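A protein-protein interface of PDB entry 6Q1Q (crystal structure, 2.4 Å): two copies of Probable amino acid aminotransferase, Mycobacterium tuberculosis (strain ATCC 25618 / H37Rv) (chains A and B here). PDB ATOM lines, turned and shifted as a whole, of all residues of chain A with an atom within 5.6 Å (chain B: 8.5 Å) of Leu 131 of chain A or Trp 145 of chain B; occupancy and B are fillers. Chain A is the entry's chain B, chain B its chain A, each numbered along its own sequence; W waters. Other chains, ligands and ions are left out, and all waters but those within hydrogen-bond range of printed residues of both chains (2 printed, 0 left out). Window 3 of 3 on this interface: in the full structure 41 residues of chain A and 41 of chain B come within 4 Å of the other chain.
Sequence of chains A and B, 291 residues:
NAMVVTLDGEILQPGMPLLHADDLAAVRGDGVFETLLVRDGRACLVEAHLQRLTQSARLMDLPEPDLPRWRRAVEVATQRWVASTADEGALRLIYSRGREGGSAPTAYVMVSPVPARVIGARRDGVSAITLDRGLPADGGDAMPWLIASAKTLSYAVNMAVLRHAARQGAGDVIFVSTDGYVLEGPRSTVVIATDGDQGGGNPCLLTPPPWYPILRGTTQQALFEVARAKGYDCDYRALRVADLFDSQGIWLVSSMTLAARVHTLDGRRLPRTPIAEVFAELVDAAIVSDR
Of the printed residues of chain B, Asp 132 of chain A touches Met 143 (3.3 Å) and Trp 145 (3.1 Å).
Of the printed residues of chain B, Ala 160 of chain A touches Trp 145 (3.96 Å) and Ile 147 (3.7 Å).
Printed residues of chain B within 4 Å of Val 161 of chain A: Trp 145 (3.8 Å).
Printed residues of chain B within 4 Å of His 164 of chain A: Trp 145.
Ala 165 of chain A touches none of the printed residues of chain B.
Leu 135 of chain B touches none of the printed residues of chain A.
Of the printed residues of chain A, Met 143 of chain B touches Asp 132 and Arg 133.
Of the printed residues of chain A, Trp 145 of chain B touches Leu 131, Asp 132, Ala 160, Val 161 and His 164.
The nearest residue of chain A that does not touch Trp 145 of chain B is Val 157 of chain A (4.4 Å).
The backbone NH of Leu 131 of chain A lies within hydrogen-bond range of the backbone carbonyl oxygen of Ile 174 of chain A (3.0 Å).
The backbone carbonyl oxygen of Leu 131 of chain A sits at hydrogen-bond distance from the backbone NH of Val 176 of chain A, at 2.9 Å.
The backbone NH of Arg 133 of chain A is in hydrogen-bond range of the backbone carbonyl oxygen of Val 176 of chain A (2.9 Å).
No position is printed for both chains.
Printed residues of chain A that touch a printed residue of chain B: Leu 131, Asp 132, Arg 133, Val 157, Ala 160, Val 161 and His 164.
Hydrophobic or aromatic side chains of chain A that line the printed part of chain B: Leu 131, Val 157, Ala 160, Val 161 and His 164.
Hydrophobic or aromatic side chains of chain B that line the printed part of chain A: Met 143, Trp 145, Leu 146 and Ile 147.
Among the printed residues, 10 pairs touch across the chains.
Among the printed residues, no Asp or Glu carboxylate lies within 4 Å of a Lys or Arg side-chain nitrogen of the other chain.
Leu 131 of chain A touches Trp 145 of chain B.
Arg 133 of chain A touches Met 143 of chain B (C to SD, 3.9 Å).
Arg 133 of chain A touches Leu 146 of chain B.
Leu 146 of chain B touches Val 157 of chain A.
Ala 160 of chain A touches Trp 145 of chain B (CB to O, 3.96 Å).
Ala 160 of chain A touches Ile 147 of chain B (CB to CD1, 3.7 Å).
Trp 145 of chain B touches Val 161 of chain A.
Trp 145 of chain B touches His 164 of chain A.
Water W2 bridges O of Ala 142 of chain B (2.9 Å) and OD1 of Asp 132 of chain A (3.3 Å).
Water W1 lies within hydrogen-bond range of N of Ala 160 of chain A (3.4 Å) and SD of Met 60 of chain B (3.7 Å).
O of Asp 132 of chain A sits at hydrogen-bond distance from NE1 of Trp 145 of chain B (3.1 Å).
The backbone carbonyl oxygen of Asp 132 of chain A lies close to the side-chain sulfur of Met 143 of chain B, at 3.3 Å.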
ATOM      1  N   ILE A 129      23.163  15.604 -36.020  1.00  0.00           N
ATOM      2  CA  ILE A 129      21.823  15.726 -36.575  1.00  0.00           C
ATOM      3  C   ILE A 129      21.497  17.205 -36.698  1.00  0.00           C
ATOM      4  O   ILE A 129      22.026  18.043 -35.960  1.00  0.00           O
ATOM      5  CB  ILE A 129      20.764  15.003 -35.718  1.00  0.00           C
ATOM      6  CG1 ILE A 129      20.789  15.534 -34.284  1.00  0.00           C
ATOM      7  CG2 ILE A 129      20.995  13.498 -35.740  1.00  0.00           C
ATOM      8  CD1 ILE A 129      19.692  14.975 -33.409  1.00  0.00           C
ATOM      9  N   THR A 130      20.637  17.525 -37.659  1.00  0.00           N
ATOM     10  CA  THR A 130      20.117  18.873 -37.804  1.00  0.00           C
ATOM     11  C   THR A 130      18.868  19.018 -36.950  1.00  0.00           C
ATOM     12  O   THR A 130      18.002  18.138 -36.946  1.00  0.00           O
ATOM     13  CB  THR A 130      19.802  19.187 -39.265  1.00  0.00           C
ATOM     14  OG1 THR A 130      18.828  18.257 -39.755  1.00  0.00           O
ATOM     15  CG2 THR A 130      21.060  19.084 -40.101  1.00  0.00           C
ATOM     16  N   LEU A 131      18.785  20.122 -36.219  1.00  0.00           N
ATOM     17  CA  LEU A 131      17.629  20.407 -35.389  1.00  0.00           C
ATOM     18  C   LEU A 131      17.176  21.836 -35.631  1.00  0.00           C
ATOM     19  O   LEU A 131      17.998  22.749 -35.773  1.00  0.00           O
ATOM     20  CB  LEU A 131      17.937  20.189 -33.899  1.00  0.00           C
ATOM     21  CG  LEU A 131      18.015  18.750 -33.379  1.00  0.00           C
ATOM     22  CD1 LEU A 131      18.549  18.714 -31.952  1.00  0.00           C
ATOM     23  CD2 LEU A 131      16.655  18.078 -33.459  1.00  0.00           C
ATOM     24  N   ASP A 132      15.863  22.019 -35.688  1.00  0.00           N
ATOM     25  CA  ASP A 132      15.311  23.350 -35.871  1.00  0.00           C
ATOM     26  C   ASP A 132      15.542  24.190 -34.627  1.00  0.00           C
ATOM     27  O   ASP A 132      15.268  23.753 -33.505  1.00  0.00           O
ATOM     28  CB  ASP A 132      13.821  23.274 -36.190  1.00  0.00           C
ATOM     29  CG  ASP A 132      13.554  22.772 -37.593  1.00  0.00           C
ATOM     30  OD1 ASP A 132      12.570  22.028 -37.785  1.00  0.00           O
ATOM     31  OD2 ASP A 132      14.339  23.111 -38.505  1.00  0.00           O
ATOM     32  N   ARG A 133      16.057  25.397 -34.832  1.00  0.00           N
ATOM     33  CA  ARG A 133      16.332  26.305 -33.732  1.00  0.00           C
ATOM     34  C   ARG A 133      15.120  27.142 -33.353  1.00  0.00           C
ATOM     35  O   ARG A 133      15.013  27.578 -32.199  1.00  0.00           O
ATOM     36  CB  ARG A 133      17.511  27.216 -34.097  1.00  0.00           C
ATOM     37  CG  ARG A 133      17.839  28.294 -33.074  1.00  0.00           C
ATOM     38  CD  ARG A 133      18.374  27.683 -31.786  1.00  0.00           C
ATOM     39  NE  ARG A 133      18.621  28.688 -30.755  1.00  0.00           N
ATOM     40  CZ  ARG A 133      17.686  29.160 -29.937  1.00  0.00           C
ATOM     41  NH1 ARG A 133      16.442  28.714 -30.026  1.00  0.00           N
ATOM     42  NH2 ARG A 133      17.993  30.074 -29.026  1.00  0.00           N
ATOM     43  N   VAL A 157      19.799  25.284 -22.225  1.00  0.00           N
ATOM     44  CA  VAL A 157      19.183  24.761 -23.441  1.00  0.00           C
ATOM     45  C   VAL A 157      20.227  24.120 -24.344  1.00  0.00           C
ATOM     46  O   VAL A 157      19.963  23.098 -24.989  1.00  0.00           O
ATOM     47  CB  VAL A 157      18.405  25.873 -24.165  1.00  0.00           C
ATOM     48  CG1 VAL A 157      17.873  25.367 -25.502  1.00  0.00           C
ATOM     49  CG2 VAL A 157      17.266  26.365 -23.290  1.00  0.00           C
ATOM     50  N   ALA A 160      20.802  20.700 -23.026  1.00  0.00           N
ATOM     51  CA  ALA A 160      19.616  19.879 -23.248  1.00  0.00           C
ATOM     52  C   ALA A 160      19.525  19.427 -24.701  1.00  0.00           C
ATOM     53  O   ALA A 160      19.076  18.310 -24.984  1.00  0.00           O
ATOM     54  CB  ALA A 160      18.359  20.647 -22.841  1.00  0.00           C
ATOM     55  N   VAL A 161      19.937  20.289 -25.634  1.00  0.00           N
ATOM     56  CA  VAL A 161      19.917  19.933 -27.051  1.00  0.00           C
ATOM     57  C   VAL A 161      20.873  18.779 -27.325  1.00  0.00           C
ATOM     58  O   VAL A 161      20.551  17.850 -28.077  1.00  0.00           O
ATOM     59  CB  VAL A 161      20.246  21.168 -27.912  1.00  0.00           C
ATOM     60  CG1 VAL A 161      20.778  20.757 -29.270  1.00  0.00           C
ATOM     61  CG2 VAL A 161      19.009  22.041 -28.072  1.00  0.00           C
ATOM     62  N   HIS A 164      19.428  15.526 -25.948  1.00  0.00           N
ATOM     63  CA  HIS A 164      18.452  15.000 -26.894  1.00  0.00           C
ATOM     64  C   HIS A 164      19.147  14.302 -28.054  1.00  0.00           C
ATOM     65  O   HIS A 164      18.788  13.177 -28.424  1.00  0.00           O
ATOM     66  CB  HIS A 164      17.555  16.129 -27.402  1.00  0.00           C
ATOM     67  CG  HIS A 164      16.633  15.713 -28.506  1.00  0.00           C
ATOM     68  ND1 HIS A 164      16.931  15.908 -29.837  1.00  0.00           N
ATOM     69  CD2 HIS A 164      15.420  15.113 -28.475  1.00  0.00           C
ATOM     70  CE1 HIS A 164      15.941  15.447 -30.579  1.00  0.00           C
ATOM     71  NE2 HIS A 164      15.011  14.960 -29.778  1.00  0.00           N
ATOM     72  N   ALA A 165      20.150  14.960 -28.644  1.00  0.00           N
ATOM     73  CA  ALA A 165      20.889  14.350 -29.745  1.00  0.00           C
ATOM     74  C   ALA A 165      21.592  13.076 -29.298  1.00  0.00           C
ATOM     75  O   ALA A 165      21.657  12.099 -30.051  1.00  0.00           O
ATOM     76  CB  ALA A 165      21.903  15.339 -30.312  1.00  0.00           C
ATOM     77  N   VAL A 173      25.042  18.608 -32.799  1.00  0.00           N
ATOM     78  CA  VAL A 173      23.844  19.163 -33.420  1.00  0.00           C
ATOM     79  C   VAL A 173      24.246  20.313 -34.331  1.00  0.00           C
ATOM     80  O   VAL A 173      25.157  21.082 -34.011  1.00  0.00           O
ATOM     81  CB  VAL A 173      22.835  19.649 -32.355  1.00  0.00           C
ATOM     82  CG1 VAL A 173      21.784  20.569 -32.967  1.00  0.00           C
ATOM     83  CG2 VAL A 173      22.174  18.479 -31.679  1.00  0.00           C
ATOM     84  N   ILE A 174      23.572  20.423 -35.473  1.00  0.00           N
ATOM     85  CA  ILE A 174      23.644  21.606 -36.321  1.00  0.00           C
ATOM     86  C   ILE A 174      22.266  22.256 -36.330  1.00  0.00           C
ATOM     87  O   ILE A 174      21.286  21.645 -36.772  1.00  0.00           O
ATOM     88  CB  ILE A 174      24.109  21.265 -37.744  1.00  0.00           C
ATOM     89  CG1 ILE A 174      25.572  20.819 -37.729  1.00  0.00           C
ATOM     90  CG2 ILE A 174      23.923  22.464 -38.654  1.00  0.00           C
ATOM     91  CD1 ILE A 174      26.143  20.551 -39.106  1.00  0.00           C
ATOM     92  N   PHE A 175      22.191  23.488 -35.836  1.00  0.00           N
ATOM     93  CA  PHE A 175      20.932  24.218 -35.793  1.00  0.00           C
ATOM     94  C   PHE A 175      20.566  24.757 -37.170  1.00  0.00           C
ATOM     95  O   PHE A 175      21.418  25.278 -37.897  1.00  0.00           O
ATOM     96  CB  PHE A 175      21.016  25.372 -34.793  1.00  0.00           C
ATOM     97  CG  PHE A 175      20.783  24.959 -33.367  1.00  0.00           C
ATOM     98  CD1 PHE A 175      19.636  24.269 -33.008  1.00  0.00           C
ATOM     99  CD2 PHE A 175      21.709  25.267 -32.383  1.00  0.00           C
ATOM    100  CE1 PHE A 175      19.418  23.890 -31.696  1.00  0.00           C
ATOM    101  CE2 PHE A 175      21.497  24.892 -31.067  1.00  0.00           C
ATOM    102  CZ  PHE A 175      20.349  24.202 -30.725  1.00  0.00           C
ATOM    103  N   VAL A 176      19.288  24.641 -37.522  1.00  0.00           N
ATOM    104  CA  VAL A 176      18.752  25.187 -38.761  1.00  0.00           C
ATOM    105  C   VAL A 176      17.665  26.196 -38.414  1.00  0.00           C
ATOM    106  O   VAL A 176      16.856  25.966 -37.508  1.00  0.00           O
ATOM    107  CB  VAL A 176      18.198  24.075 -39.678  1.00  0.00           C
ATOM    108  CG1 VAL A 176      17.628  24.667 -40.962  1.00  0.00           C
ATOM    109  CG2 VAL A 176      19.283  23.058 -39.987  1.00  0.00           C
ATOM    110  N   LEU B  59      12.355  17.351 -17.186  1.00  0.00           N
ATOM    111  CA  LEU B  59      12.677  17.892 -18.503  1.00  0.00           C
ATOM    112  C   LEU B  59      14.163  18.179 -18.645  1.00  0.00           C
ATOM    113  O   LEU B  59      14.678  18.197 -19.769  1.00  0.00           O
ATOM    114  CB  LEU B  59      11.892  19.178 -18.765  1.00  0.00           C
ATOM    115  CG  LEU B  59      10.374  19.114 -18.928  1.00  0.00           C
ATOM    116  CD1 LEU B  59       9.774  20.497 -18.718  1.00  0.00           C
ATOM    117  CD2 LEU B  59      10.004  18.567 -20.301  1.00  0.00           C
ATOM    118  N   MET B  60      14.864  18.382 -17.531  1.00  0.00           N
ATOM    119  CA  MET B  60      16.287  18.685 -17.521  1.00  0.00           C
ATOM    120  C   MET B  60      17.147  17.463 -17.230  1.00  0.00           C
ATOM    121  O   MET B  60      18.355  17.609 -17.003  1.00  0.00           O
ATOM    122  CB  MET B  60      16.574  19.777 -16.491  1.00  0.00           C
ATOM    123  CG  MET B  60      16.240  21.176 -16.968  1.00  0.00           C
ATOM    124  SD  MET B  60      17.572  21.874 -17.956  1.00  0.00           S
ATOM    125  CE  MET B  60      18.708  22.380 -16.668  1.00  0.00           C
ATOM    126  N   LEU B 135      10.417  32.505 -31.046  1.00  0.00           N
ATOM    127  CA  LEU B 135       9.877  31.169 -31.138  1.00  0.00           C
ATOM    128  C   LEU B 135       8.485  31.207 -31.758  1.00  0.00           C
ATOM    129  O   LEU B 135       7.725  32.144 -31.492  1.00  0.00           O
ATOM    130  CB  LEU B 135       9.811  30.525 -29.744  1.00  0.00           C
ATOM    131  CG  LEU B 135      11.149  30.024 -29.198  1.00  0.00           C
ATOM    132  CD1 LEU B 135      10.961  29.315 -27.863  1.00  0.00           C
ATOM    133  CD2 LEU B 135      11.840  29.116 -30.200  1.00  0.00           C
ATOM    134  N   GLY B 139       6.187  25.997 -31.558  1.00  0.00           N
ATOM    135  CA  GLY B 139       7.553  25.569 -31.309  1.00  0.00           C
ATOM    136  C   GLY B 139       7.657  24.573 -30.170  1.00  0.00           C
ATOM    137  O   GLY B 139       8.513  23.685 -30.187  1.00  0.00           O
ATOM    138  N   GLY B 140       6.809  24.725 -29.149  1.00  0.00           N
ATOM    139  CA  GLY B 140       6.866  23.824 -28.010  1.00  0.00           C
ATOM    140  C   GLY B 140       6.651  22.376 -28.409  1.00  0.00           C
ATOM    141  O   GLY B 140       7.330  21.475 -27.910  1.00  0.00           O
ATOM    142  N   ASP B 141       5.705  22.136 -29.316  1.00  0.00           N
ATOM    143  CA  ASP B 141       5.437  20.784 -29.790  1.00  0.00           C
ATOM    144  C   ASP B 141       6.506  20.322 -30.773  1.00  0.00           C
ATOM    145  O   ASP B 141       7.003  19.195 -30.681  1.00  0.00           O
ATOM    146  CB  ASP B 141       4.054  20.724 -30.443  1.00  0.00           C
ATOM    147  CG  ASP B 141       2.925  20.735 -29.429  1.00  0.00           C
ATOM    148  OD1 ASP B 141       3.200  20.599 -28.215  1.00  0.00           O
ATOM    149  OD2 ASP B 141       1.759  20.887 -29.851  1.00  0.00           O
ATOM    150  N   ALA B 142       6.877  21.185 -31.721  1.00  0.00           N
ATOM    151  CA  ALA B 142       7.766  20.758 -32.795  1.00  0.00           C
ATOM    152  C   ALA B 142       9.200  20.573 -32.310  1.00  0.00           C
ATOM    153  O   ALA B 142       9.960  19.808 -32.913  1.00  0.00           O
ATOM    154  CB  ALA B 142       7.720  21.764 -33.944  1.00  0.00           C
ATOM    155  N   MET B 143       9.597  21.275 -31.248  1.00  0.00           N
ATOM    156  CA  MET B 143      10.981  21.291 -30.772  1.00  0.00           C
ATOM    157  C   MET B 143      11.027  21.059 -29.266  1.00  0.00           C
ATOM    158  O   MET B 143      11.230  22.000 -28.486  1.00  0.00           O
ATOM    159  CB  MET B 143      11.666  22.607 -31.141  1.00  0.00           C
ATOM    160  CG  MET B 143      11.133  23.237 -32.417  1.00  0.00           C
ATOM    161  SD  MET B 143      12.145  24.599 -33.005  1.00  0.00           S
ATOM    162  CE  MET B 143      11.316  25.935 -32.162  1.00  0.00           C
ATOM    163  N   PRO B 144      10.855  19.811 -28.818  1.00  0.00           N
ATOM    164  CA  PRO B 144      10.937  19.542 -27.372  1.00  0.00           C
ATOM    165  C   PRO B 144      12.341  19.691 -26.813  1.00  0.00           C
ATOM    166  O   PRO B 144      12.489  19.862 -25.599  1.00  0.00           O
ATOM    167  CB  PRO B 144      10.431  18.099 -27.253  1.00  0.00           C
ATOM    168  CG  PRO B 144      10.728  17.492 -28.588  1.00  0.00           C
ATOM    169  CD  PRO B 144      10.555  18.595 -29.595  1.00  0.00           C
ATOM    170  N   TRP B 145      13.372  19.641 -27.658  1.00  0.00           N
ATOM    171  CA  TRP B 145      14.743  19.813 -27.195  1.00  0.00           C
ATOM    172  C   TRP B 145      15.012  21.210 -26.648  1.00  0.00           C
ATOM    173  O   TRP B 145      15.996  21.396 -25.924  1.00  0.00           O
ATOM    174  CB  TRP B 145      15.717  19.487 -28.327  1.00  0.00           C
ATOM    175  CG  TRP B 145      15.357  20.115 -29.643  1.00  0.00           C
ATOM    176  CD1 TRP B 145      15.738  21.343 -30.100  1.00  0.00           C
ATOM    177  CD2 TRP B 145      14.552  19.533 -30.679  1.00  0.00           C
ATOM    178  NE1 TRP B 145      15.218  21.565 -31.354  1.00  0.00           N
ATOM    179  CE2 TRP B 145      14.487  20.468 -31.732  1.00  0.00           C
ATOM    180  CE3 TRP B 145      13.881  18.313 -30.817  1.00  0.00           C
ATOM    181  CZ2 TRP B 145      13.775  20.223 -32.908  1.00  0.00           C
ATOM    182  CZ3 TRP B 145      13.174  18.071 -31.984  1.00  0.00           C
ATOM    183  CH2 TRP B 145      13.128  19.023 -33.015  1.00  0.00           C
ATOM    184  N   LEU B 146      14.184  22.200 -26.985  1.00  0.00           N
ATOM    185  CA  LEU B 146      14.342  23.530 -26.412  1.00  0.00           C
ATOM    186  C   LEU B 146      13.836  23.637 -24.979  1.00  0.00           C
ATOM    187  O   LEU B 146      14.030  24.691 -24.363  1.00  0.00           O
ATOM    188  CB  LEU B 146      13.645  24.581 -27.278  1.00  0.00           C
ATOM    189  CG  LEU B 146      14.238  24.764 -28.676  1.00  0.00           C
ATOM    190  CD1 LEU B 146      13.590  25.944 -29.378  1.00  0.00           C
ATOM    191  CD2 LEU B 146      15.745  24.956 -28.585  1.00  0.00           C
ATOM    192  N   ILE B 147      13.186  22.595 -24.450  1.00  0.00           N
ATOM    193  CA  ILE B 147      12.751  22.493 -23.052  1.00  0.00           C
ATOM    194  C   ILE B 147      12.115  23.792 -22.565  1.00  0.00           C
ATOM    195  O   ILE B 147      12.367  24.244 -21.444  1.00  0.00           O
ATOM    196  CB  ILE B 147      13.909  22.054 -22.126  1.00  0.00           C
ATOM    197  CG1 ILE B 147      15.031  23.094 -22.041  1.00  0.00           C
ATOM    198  CG2 ILE B 147      14.477  20.719 -22.584  1.00  0.00           C
ATOM    199  CD1 ILE B 147      16.031  22.815 -20.961  1.00  0.00           C
ATOM    200  N   ALA B 148      11.251  24.378 -23.395  1.00  0.00           N
ATOM    201  CA  ALA B 148      10.673  25.679 -23.082  1.00  0.00           C
ATOM    202  C   ALA B 148       9.781  25.654 -21.847  1.00  0.00           C
ATOM    203  O   ALA B 148       9.510  26.715 -21.275  1.00  0.00           O
ATOM    204  CB  ALA B 148       9.879  26.198 -24.279  1.00  0.00           C
ATOM    205  N   SER B 149       9.305  24.483 -21.431  1.00  0.00           N
ATOM    206  CA  SER B 149       8.456  24.377 -20.253  1.00  0.00           C
ATOM    207  C   SER B 149       9.242  24.185 -18.963  1.00  0.00           C
ATOM    208  O   SER B 149       8.639  24.168 -17.886  1.00  0.00           O
ATOM    209  CB  SER B 149       7.461  23.226 -20.422  1.00  0.00           C
ATOM    210  OG  SER B 149       6.462  23.565 -21.365  1.00  0.00           O
HETATM  211  O   HOH W   1      20.864  21.472 -19.675  1.00  0.00           O
HETATM  212  O   HOH W   2      11.086  20.157 -35.550  1.00  0.00           O
